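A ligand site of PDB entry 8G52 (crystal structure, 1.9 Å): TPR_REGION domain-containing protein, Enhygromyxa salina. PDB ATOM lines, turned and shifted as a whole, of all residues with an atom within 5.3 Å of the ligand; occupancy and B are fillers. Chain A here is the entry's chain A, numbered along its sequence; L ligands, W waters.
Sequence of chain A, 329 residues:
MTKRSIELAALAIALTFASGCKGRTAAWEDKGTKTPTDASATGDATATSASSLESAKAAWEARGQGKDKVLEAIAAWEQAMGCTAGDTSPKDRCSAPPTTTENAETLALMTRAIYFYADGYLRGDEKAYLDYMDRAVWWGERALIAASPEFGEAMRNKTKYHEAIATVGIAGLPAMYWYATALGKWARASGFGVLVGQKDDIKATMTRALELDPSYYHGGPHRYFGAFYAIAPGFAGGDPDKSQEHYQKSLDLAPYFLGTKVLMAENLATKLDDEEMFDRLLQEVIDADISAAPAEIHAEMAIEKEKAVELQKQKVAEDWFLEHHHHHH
Thr 181 touches the ligand (CG2 to C4, 3.6 Å). CA of Gly 184 touches C8 of the ligand, at 3.8 Å. CG of Lys 185 touches C6 of the ligand (3.997 Å). Phe 192 touches the ligand. Leu 195 touches the ligand. CG1 of Val 196 touches C16 of the ligand, 3.8 Å away. CB of Lys 199 touches C14 of the ligand, at 3.6 Å. Tyr 217 touches the ligand. Tyr 224 touches the ligand (OH to C8, 3.6 Å). CB of Ala 227 touches C7 of the ligand, 3.99 Å away. CD2 of Phe 228 touches C12 of the ligand (3.97 Å). Ile 231 touches the ligand. Ala 232 touches the ligand (CA to C16, 3.6 Å). CD of Pro 233 touches C16 of the ligand, at 3.3 Å. CB of Ala 236 touches C16 of the ligand, at 3.9 Å. Hydrophobic or aromatic side chains that line the ligand: Tyr 177, Phe 192, Leu 195, Val 196, Tyr 217, Tyr 224, Ala 227, Phe 228, Ile 231, Ala 232, Pro 233 and Ala 236. Within 4 Å of the ligand: Tyr 177, Thr 181, Gly 184, Lys 185, Phe 192, Leu 195, Val 196, Lys 199, Tyr 217, Arg 223, Tyr 224, Ala 227, Phe 228, Ile 231, Ala 232, Pro 233 and Ala 236.
The side-chain hydroxyl of Tyr 177 lies within hydrogen-bond range of an oxygen (O2) of the ligand (2.6 Å). O2 of the ligand is in salt-bridge range of NH2 of Arg 223.
The backbone carbonyl oxygen (O) of Tyr 177 is in hydrogen-bond range of the side-chain hydroxyl (OG1) of Thr 181 (3.0 Å). The backbone carbonyl oxygen (O) of Gly 220 sits at hydrogen-bond distance from the side-chain hydroxyl (OH) of Tyr 177 (3.3 Å). NH2 of Arg 223 lies within hydrogen-bond range of O of Tyr 217. The side-chain hydroxyl of Tyr 224 is in hydrogen-bond range of the backbone carbonyl oxygen of Ala 180 (2.7 Å). The side-chain amino group (NZ) of Lys 185 sits close to the side-chain hydroxyl (OH) of Tyr 115, 3.3 Å away.
Water W2 bridges an oxygen (O1) of the ligand (2.7 Å) and the side-chain hydroxyl of Tyr 217 (2.7 Å). Water W3 bridges OH of Tyr 115 (2.6 Å) and O1 of the ligand (2.7 Å).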
ATOM      1  N   TYR A 115     -26.017   4.517  11.687  1.00  0.00           N
ATOM      2  CA  TYR A 115     -25.625   4.380  13.081  1.00  0.00           C
ATOM      3  C   TYR A 115     -26.373   3.238  13.768  1.00  0.00           C
ATOM      4  O   TYR A 115     -25.754   2.391  14.420  1.00  0.00           O
ATOM      5  CB  TYR A 115     -25.866   5.696  13.844  1.00  0.00           C
ATOM      6  CG  TYR A 115     -25.756   5.514  15.340  1.00  0.00           C
ATOM      7  CD1 TYR A 115     -24.520   5.516  15.953  1.00  0.00           C
ATOM      8  CD2 TYR A 115     -26.882   5.303  16.123  1.00  0.00           C
ATOM      9  CE1 TYR A 115     -24.403   5.326  17.334  1.00  0.00           C
ATOM     10  CE2 TYR A 115     -26.794   5.100  17.485  1.00  0.00           C
ATOM     11  CZ  TYR A 115     -25.542   5.109  18.100  1.00  0.00           C
ATOM     12  OH  TYR A 115     -25.444   4.925  19.435  1.00  0.00           O
ATOM     13  N   TYR A 177     -27.459  16.085  15.884  1.00  0.00           N
ATOM     14  CA  TYR A 177     -27.464  15.073  16.945  1.00  0.00           C
ATOM     15  C   TYR A 177     -26.977  13.725  16.427  1.00  0.00           C
ATOM     16  O   TYR A 177     -26.121  13.073  17.046  1.00  0.00           O
ATOM     17  CB  TYR A 177     -28.860  14.949  17.556  1.00  0.00           C
ATOM     18  CG  TYR A 177     -28.872  13.956  18.709  1.00  0.00           C
ATOM     19  CD1 TYR A 177     -28.410  14.340  19.983  1.00  0.00           C
ATOM     20  CD2 TYR A 177     -29.299  12.652  18.546  1.00  0.00           C
ATOM     21  CE1 TYR A 177     -28.373  13.453  21.015  1.00  0.00           C
ATOM     22  CE2 TYR A 177     -29.280  11.748  19.611  1.00  0.00           C
ATOM     23  CZ  TYR A 177     -28.801  12.170  20.845  1.00  0.00           C
ATOM     24  OH  TYR A 177     -28.740  11.277  21.932  1.00  0.00           O
ATOM     25  N   TRP A 178     -27.498  13.277  15.299  1.00  0.00           N
ATOM     26  CA  TRP A 178     -27.102  11.958  14.784  1.00  0.00           C
ATOM     27  C   TRP A 178     -25.729  11.987  14.147  1.00  0.00           C
ATOM     28  O   TRP A 178     -25.065  10.951  14.088  1.00  0.00           O
ATOM     29  CB  TRP A 178     -28.180  11.443  13.811  1.00  0.00           C
ATOM     30  CG  TRP A 178     -29.391  11.117  14.592  1.00  0.00           C
ATOM     31  CD1 TRP A 178     -30.561  11.815  14.615  1.00  0.00           C
ATOM     32  CD2 TRP A 178     -29.528  10.047  15.547  1.00  0.00           C
ATOM     33  NE1 TRP A 178     -31.423  11.244  15.512  1.00  0.00           N
ATOM     34  CE2 TRP A 178     -30.822  10.158  16.098  1.00  0.00           C
ATOM     35  CE3 TRP A 178     -28.698   9.008  15.969  1.00  0.00           C
ATOM     36  CZ2 TRP A 178     -31.312   9.247  17.045  1.00  0.00           C
ATOM     37  CZ3 TRP A 178     -29.181   8.106  16.925  1.00  0.00           C
ATOM     38  CH2 TRP A 178     -30.475   8.228  17.454  1.00  0.00           C
ATOM     39  N   ALA A 180     -23.250  13.790  15.460  1.00  0.00           N
ATOM     40  CA  ALA A 180     -22.387  13.740  16.639  1.00  0.00           C
ATOM     41  C   ALA A 180     -22.391  12.355  17.284  1.00  0.00           C
ATOM     42  O   ALA A 180     -21.378  11.926  17.854  1.00  0.00           O
ATOM     43  CB  ALA A 180     -22.852  14.800  17.633  1.00  0.00           C
ATOM     44  N   THR A 181     -23.527  11.674  17.232  1.00  0.00           N
ATOM     45  CA  THR A 181     -23.614  10.301  17.752  1.00  0.00           C
ATOM     46  C   THR A 181     -22.739   9.359  16.948  1.00  0.00           C
ATOM     47  O   THR A 181     -21.939   8.598  17.536  1.00  0.00           O
ATOM     48  CB  THR A 181     -25.076   9.876  17.739  1.00  0.00           C
ATOM     49  OG1 THR A 181     -25.786  10.641  18.728  1.00  0.00           O
ATOM     50  CG2 THR A 181     -25.253   8.419  18.025  1.00  0.00           C
ATOM     51  N   GLY A 184     -18.984  10.471  17.437  1.00  0.00           N
ATOM     52  CA  GLY A 184     -18.485  10.067  18.739  1.00  0.00           C
ATOM     53  C   GLY A 184     -18.222   8.581  18.834  1.00  0.00           C
ATOM     54  O   GLY A 184     -17.179   8.148  19.360  1.00  0.00           O
ATOM     55  N   LYS A 185     -19.161   7.761  18.353  1.00  0.00           N
ATOM     56  CA  LYS A 185     -18.922   6.320  18.471  1.00  0.00           C
ATOM     57  C   LYS A 185     -17.853   5.875  17.487  1.00  0.00           C
ATOM     58  O   LYS A 185     -17.076   4.955  17.797  1.00  0.00           O
ATOM     59  CB  LYS A 185     -20.204   5.543  18.303  1.00  0.00           C
ATOM     60  CG  LYS A 185     -21.177   5.767  19.438  1.00  0.00           C
ATOM     61  CD  LYS A 185     -21.855   4.457  19.844  1.00  0.00           C
ATOM     62  CE  LYS A 185     -22.851   4.707  20.975  1.00  0.00           C
ATOM     63  NZ  LYS A 185     -23.395   3.463  21.559  1.00  0.00           N
ATOM     64  N   ARG A 188     -14.575   6.973  19.242  1.00  0.00           N
ATOM     65  CA  ARG A 188     -14.293   6.141  20.403  1.00  0.00           C
ATOM     66  C   ARG A 188     -13.690   4.804  19.981  1.00  0.00           C
ATOM     67  O   ARG A 188     -12.697   4.338  20.569  1.00  0.00           O
ATOM     68  CB  ARG A 188     -15.573   5.901  21.220  1.00  0.00           C
ATOM     69  CG  ARG A 188     -15.267   5.321  22.614  1.00  0.00           C
ATOM     70  CD  ARG A 188     -16.471   5.286  23.539  1.00  0.00           C
ATOM     71  NE  ARG A 188     -16.173   4.680  24.838  1.00  0.00           N
ATOM     72  CZ  ARG A 188     -17.097   4.238  25.678  1.00  0.00           C
ATOM     73  NH1 ARG A 188     -18.388   4.258  25.358  1.00  0.00           N
ATOM     74  NH2 ARG A 188     -16.735   3.796  26.881  1.00  0.00           N
ATOM     75  N   PHE A 192      -7.798   6.632  21.339  1.00  0.00           N
ATOM     76  CA  PHE A 192      -7.786   7.871  22.118  1.00  0.00           C
ATOM     77  C   PHE A 192      -7.349   9.066  21.281  1.00  0.00           C
ATOM     78  O   PHE A 192      -7.879  10.171  21.446  1.00  0.00           O
ATOM     79  CB  PHE A 192      -6.869   7.706  23.338  1.00  0.00           C
ATOM     80  CG  PHE A 192      -6.990   8.834  24.314  1.00  0.00           C
ATOM     81  CD1 PHE A 192      -8.155   9.024  25.014  1.00  0.00           C
ATOM     82  CD2 PHE A 192      -5.936   9.711  24.515  1.00  0.00           C
ATOM     83  CE1 PHE A 192      -8.290  10.076  25.902  1.00  0.00           C
ATOM     84  CE2 PHE A 192      -6.068  10.752  25.411  1.00  0.00           C
ATOM     85  CZ  PHE A 192      -7.254  10.937  26.099  1.00  0.00           C
ATOM     86  N   LEU A 195     -10.224  10.142  19.294  1.00  0.00           N
ATOM     87  CA  LEU A 195     -11.276  10.629  20.166  1.00  0.00           C
ATOM     88  C   LEU A 195     -10.985  12.053  20.654  1.00  0.00           C
ATOM     89  O   LEU A 195     -11.842  12.932  20.545  1.00  0.00           O
ATOM     90  CB  LEU A 195     -11.449   9.680  21.358  1.00  0.00           C
ATOM     91  CG  LEU A 195     -12.682   9.847  22.253  1.00  0.00           C
ATOM     92  CD1 LEU A 195     -13.978   9.659  21.478  1.00  0.00           C
ATOM     93  CD2 LEU A 195     -12.593   8.832  23.398  1.00  0.00           C
ATOM     94  N   VAL A 196      -9.796  12.283  21.205  1.00  0.00           N
ATOM     95  CA  VAL A 196      -9.502  13.602  21.745  1.00  0.00           C
ATOM     96  C   VAL A 196      -9.407  14.627  20.616  1.00  0.00           C
ATOM     97  O   VAL A 196      -9.637  15.827  20.834  1.00  0.00           O
ATOM     98  CB  VAL A 196      -8.205  13.613  22.572  1.00  0.00           C
ATOM     99  CG1 VAL A 196      -8.278  12.575  23.647  1.00  0.00           C
ATOM    100  CG2 VAL A 196      -6.999  13.391  21.671  1.00  0.00           C
ATOM    101  N   LYS A 199     -12.942  15.942  20.239  1.00  0.00           N
ATOM    102  CA  LYS A 199     -13.660  16.270  21.469  1.00  0.00           C
ATOM    103  C   LYS A 199     -14.301  17.654  21.407  1.00  0.00           C
ATOM    104  O   LYS A 199     -15.455  17.831  21.820  1.00  0.00           O
ATOM    105  CB  LYS A 199     -12.688  16.186  22.656  1.00  0.00           C
ATOM    106  CG  LYS A 199     -13.079  17.017  23.862  1.00  0.00           C
ATOM    107  CD  LYS A 199     -12.091  16.849  25.024  1.00  0.00           C
ATOM    108  CE  LYS A 199     -10.739  17.503  24.753  1.00  0.00           C
ATOM    109  NZ  LYS A 199     -10.756  18.949  25.106  1.00  0.00           N
ATOM    110  N   ILE A 202     -17.179  17.849  18.857  1.00  0.00           N
ATOM    111  CA  ILE A 202     -18.327  17.139  19.408  1.00  0.00           C
ATOM    112  C   ILE A 202     -19.013  17.999  20.460  1.00  0.00           C
ATOM    113  O   ILE A 202     -20.236  18.198  20.440  1.00  0.00           O
ATOM    114  CB  ILE A 202     -17.896  15.773  19.969  1.00  0.00           C
ATOM    115  CG1 ILE A 202     -17.723  14.763  18.836  1.00  0.00           C
ATOM    116  CG2 ILE A 202     -18.905  15.292  21.001  1.00  0.00           C
ATOM    117  CD1 ILE A 202     -16.986  13.510  19.219  1.00  0.00           C
ATOM    118  N   TYR A 217     -35.279  13.806  21.036  1.00  0.00           N
ATOM    119  CA  TYR A 217     -35.097  12.353  21.020  1.00  0.00           C
ATOM    120  C   TYR A 217     -34.880  11.832  22.446  1.00  0.00           C
ATOM    121  O   TYR A 217     -33.854  11.255  22.790  1.00  0.00           O
ATOM    122  CB  TYR A 217     -33.955  11.951  20.093  1.00  0.00           C
ATOM    123  CG  TYR A 217     -33.797  10.437  19.914  1.00  0.00           C
ATOM    124  CD1 TYR A 217     -34.769   9.702  19.253  1.00  0.00           C
ATOM    125  CD2 TYR A 217     -32.695   9.755  20.418  1.00  0.00           C
ATOM    126  CE1 TYR A 217     -34.656   8.331  19.092  1.00  0.00           C
ATOM    127  CE2 TYR A 217     -32.569   8.370  20.281  1.00  0.00           C
ATOM    128  CZ  TYR A 217     -33.569   7.672  19.621  1.00  0.00           C
ATOM    129  OH  TYR A 217     -33.508   6.313  19.435  1.00  0.00           O
ATOM    130  N   GLY A 220     -32.053  13.230  24.605  1.00  0.00           N
ATOM    131  CA  GLY A 220     -30.817  12.859  23.936  1.00  0.00           C
ATOM    132  C   GLY A 220     -29.617  13.731  24.246  1.00  0.00           C
ATOM    133  O   GLY A 220     -28.546  13.227  24.561  1.00  0.00           O
ATOM    134  N   ARG A 223     -28.412  12.847  27.666  1.00  0.00           N
ATOM    135  CA  ARG A 223     -27.835  11.511  27.657  1.00  0.00           C
ATOM    136  C   ARG A 223     -26.462  11.500  26.976  1.00  0.00           C
ATOM    137  O   ARG A 223     -25.523  10.856  27.447  1.00  0.00           O
ATOM    138  CB  ARG A 223     -28.773  10.515  26.940  1.00  0.00           C
ATOM    139  CG  ARG A 223     -28.119   9.187  26.535  1.00  0.00           C
ATOM    140  CD  ARG A 223     -29.143   8.161  26.024  1.00  0.00           C
ATOM    141  NE  ARG A 223     -29.876   8.622  24.847  1.00  0.00           N
ATOM    142  CZ  ARG A 223     -31.069   9.201  24.888  1.00  0.00           C
ATOM    143  NH1 ARG A 223     -31.709   9.433  26.026  1.00  0.00           N
ATOM    144  NH2 ARG A 223     -31.646   9.535  23.743  1.00  0.00           N
ATOM    145  N   TYR A 224     -26.331  12.250  25.871  1.00  0.00           N
ATOM    146  CA  TYR A 224     -25.049  12.342  25.172  1.00  0.00           C
ATOM    147  C   TYR A 224     -23.985  12.934  26.084  1.00  0.00           C
ATOM    148  O   TYR A 224     -22.868  12.398  26.171  1.00  0.00           O
ATOM    149  CB  TYR A 224     -25.213  13.194  23.890  1.00  0.00           C
ATOM    150  CG  TYR A 224     -24.062  13.058  22.921  1.00  0.00           C
ATOM    151  CD1 TYR A 224     -22.812  13.549  23.251  1.00  0.00           C
ATOM    152  CD2 TYR A 224     -24.227  12.422  21.687  1.00  0.00           C
ATOM    153  CE1 TYR A 224     -21.755  13.419  22.392  1.00  0.00           C
ATOM    154  CE2 TYR A 224     -23.178  12.285  20.819  1.00  0.00           C
ATOM    155  CZ  TYR A 224     -21.924  12.794  21.186  1.00  0.00           C
ATOM    156  OH  TYR A 224     -20.829  12.696  20.356  1.00  0.00           O
ATOM    157  N   ALA A 227     -22.533  10.621  28.728  1.00  0.00           N
ATOM    158  CA  ALA A 227     -21.441   9.827  28.185  1.00  0.00           C
ATOM    159  C   ALA A 227     -20.207  10.661  27.924  1.00  0.00           C
ATOM    160  O   ALA A 227     -19.094  10.220  28.212  1.00  0.00           O
ATOM    161  CB  ALA A 227     -21.897   9.134  26.900  1.00  0.00           C
ATOM    162  N   PHE A 228     -20.367  11.864  27.377  1.00  0.00           N
ATOM    163  CA  PHE A 228     -19.224  12.719  27.083  1.00  0.00           C
ATOM    164  C   PHE A 228     -18.366  12.945  28.339  1.00  0.00           C
ATOM    165  O   PHE A 228     -17.144  12.789  28.307  1.00  0.00           O
ATOM    166  CB  PHE A 228     -19.721  14.058  26.524  1.00  0.00           C
ATOM    167  CG  PHE A 228     -18.644  15.043  26.187  1.00  0.00           C
ATOM    168  CD1 PHE A 228     -18.115  15.883  27.176  1.00  0.00           C
ATOM    169  CD2 PHE A 228     -18.143  15.134  24.895  1.00  0.00           C
ATOM    170  CE1 PHE A 228     -17.114  16.791  26.874  1.00  0.00           C
ATOM    171  CE2 PHE A 228     -17.161  16.036  24.569  1.00  0.00           C
ATOM    172  CZ  PHE A 228     -16.629  16.865  25.565  1.00  0.00           C
ATOM    173  N   ILE A 231     -16.723   9.512  29.638  1.00  0.00           N
ATOM    174  CA  ILE A 231     -15.723   8.893  28.764  1.00  0.00           C
ATOM    175  C   ILE A 231     -14.435   9.696  28.753  1.00  0.00           C
ATOM    176  O   ILE A 231     -13.336   9.145  28.801  1.00  0.00           O
ATOM    177  CB  ILE A 231     -16.308   8.737  27.333  1.00  0.00           C
ATOM    178  CG1 ILE A 231     -17.379   7.653  27.275  1.00  0.00           C
ATOM    179  CG2 ILE A 231     -15.171   8.430  26.355  1.00  0.00           C
ATOM    180  CD1 ILE A 231     -18.339   7.727  26.018  1.00  0.00           C
ATOM    181  N   ALA A 232     -14.548  11.014  28.712  1.00  0.00           N
ATOM    182  CA  ALA A 232     -13.350  11.848  28.668  1.00  0.00           C
ATOM    183  C   ALA A 232     -12.564  11.708  29.977  1.00  0.00           C
ATOM    184  O   ALA A 232     -13.159  11.728  31.060  1.00  0.00           O
ATOM    185  CB  ALA A 232     -13.718  13.310  28.444  1.00  0.00           C
ATOM    186  N   PRO A 233     -11.241  11.552  29.915  1.00  0.00           N
ATOM    187  CA  PRO A 233     -10.451  11.579  31.144  1.00  0.00           C
ATOM    188  C   PRO A 233     -10.510  12.951  31.799  1.00  0.00           C
ATOM    189  O   PRO A 233     -10.766  13.964  31.147  1.00  0.00           O
ATOM    190  CB  PRO A 233      -9.027  11.262  30.664  1.00  0.00           C
ATOM    191  CG  PRO A 233      -9.204  10.612  29.327  1.00  0.00           C
ATOM    192  CD  PRO A 233     -10.400  11.318  28.731  1.00  0.00           C
ATOM    193  N   ALA A 236      -8.789  15.716  30.165  1.00  0.00           N
ATOM    194  CA  ALA A 236      -9.328  16.077  28.868  1.00  0.00           C
ATOM    195  C   ALA A 236     -10.727  16.679  28.962  1.00  0.00           C
ATOM    196  O   ALA A 236     -11.436  16.771  27.943  1.00  0.00           O
ATOM    197  CB  ALA A 236      -9.360  14.848  27.948  1.00  0.00           C
ATOM    198  N   PHE A 257     -36.249   5.677  28.588  1.00  0.00           N
ATOM    199  CA  PHE A 257     -35.217   5.436  27.581  1.00  0.00           C
ATOM    200  C   PHE A 257     -34.103   4.593  28.204  1.00  0.00           C
ATOM    201  O   PHE A 257     -33.210   5.099  28.887  1.00  0.00           O
ATOM    202  CB  PHE A 257     -34.671   6.730  27.003  1.00  0.00           C
ATOM    203  CG  PHE A 257     -34.037   6.548  25.662  1.00  0.00           C
ATOM    204  CD1 PHE A 257     -34.812   6.587  24.508  1.00  0.00           C
ATOM    205  CD2 PHE A 257     -32.681   6.273  25.557  1.00  0.00           C
ATOM    206  CE1 PHE A 257     -34.228   6.402  23.257  1.00  0.00           C
ATOM    207  CE2 PHE A 257     -32.096   6.077  24.329  1.00  0.00           C
ATOM    208  CZ  PHE A 257     -32.861   6.145  23.162  1.00  0.00           C
ATOM    209  N   LEU A 263     -25.636   3.255  28.891  1.00  0.00           N
ATOM    210  CA  LEU A 263     -24.455   4.105  28.800  1.00  0.00           C
ATOM    211  C   LEU A 263     -23.896   4.402  30.189  1.00  0.00           C
ATOM    212  O   LEU A 263     -22.685   4.395  30.371  1.00  0.00           O
ATOM    213  CB  LEU A 263     -24.776   5.402  28.061  1.00  0.00           C
ATOM    214  CG  LEU A 263     -24.985   5.289  26.540  1.00  0.00           C
ATOM    215  CD1 LEU A 263     -25.726   6.527  26.011  1.00  0.00           C
ATOM    216  CD2 LEU A 263     -23.665   5.106  25.850  1.00  0.00           C
HETATM  217  C1  LIG L   1     -28.872   7.838  21.500  1.00  0.00           C
HETATM  218  O1  LIG L   1     -29.198   6.579  21.472  1.00  0.00           O
HETATM  219  O2  LIG L   1     -29.522   8.847  21.929  1.00  0.00           O
HETATM  220  C2  LIG L   1     -27.436   8.155  20.981  1.00  0.00           C
HETATM  221  C3  LIG L   1     -26.352   8.346  22.110  1.00  0.00           C
HETATM  222  C4  LIG L   1     -24.903   8.518  21.581  1.00  0.00           C
HETATM  223  C5  LIG L   1     -23.791   8.499  22.666  1.00  0.00           C
HETATM  224  C6  LIG L   1     -22.337   8.538  22.074  1.00  0.00           C
HETATM  225  C7  LIG L   1     -21.273   9.163  22.956  1.00  0.00           C
HETATM  226  C8  LIG L   1     -20.025   9.736  22.196  1.00  0.00           C
HETATM  227  C9  LIG L   1     -18.733   9.879  23.085  1.00  0.00           C
HETATM  228  C10 LIG L   1     -17.881  11.205  22.894  1.00  0.00           C
HETATM  229  C11 LIG L   1     -16.809  11.368  24.013  1.00  0.00           C
HETATM  230  C12 LIG L   1     -15.635  12.299  23.689  1.00  0.00           C
HETATM  231  C13 LIG L   1     -14.470  12.149  24.693  1.00  0.00           C
HETATM  232  C14 LIG L   1     -13.551  13.368  24.776  1.00  0.00           C
HETATM  233  C15 LIG L   1     -12.072  13.030  24.546  1.00  0.00           C
HETATM  234  C16 LIG L   1     -11.404  12.326  25.734  1.00  0.00           C
HETATM  235  O   HOH W   1     -28.911   4.935  23.759  1.00  0.00           O
HETATM  236  O   HOH W   2     -31.124   5.236  20.211  1.00  0.00           O
HETATM  237  O   HOH W   3     -27.609   4.522  20.780  1.00  0.00           O
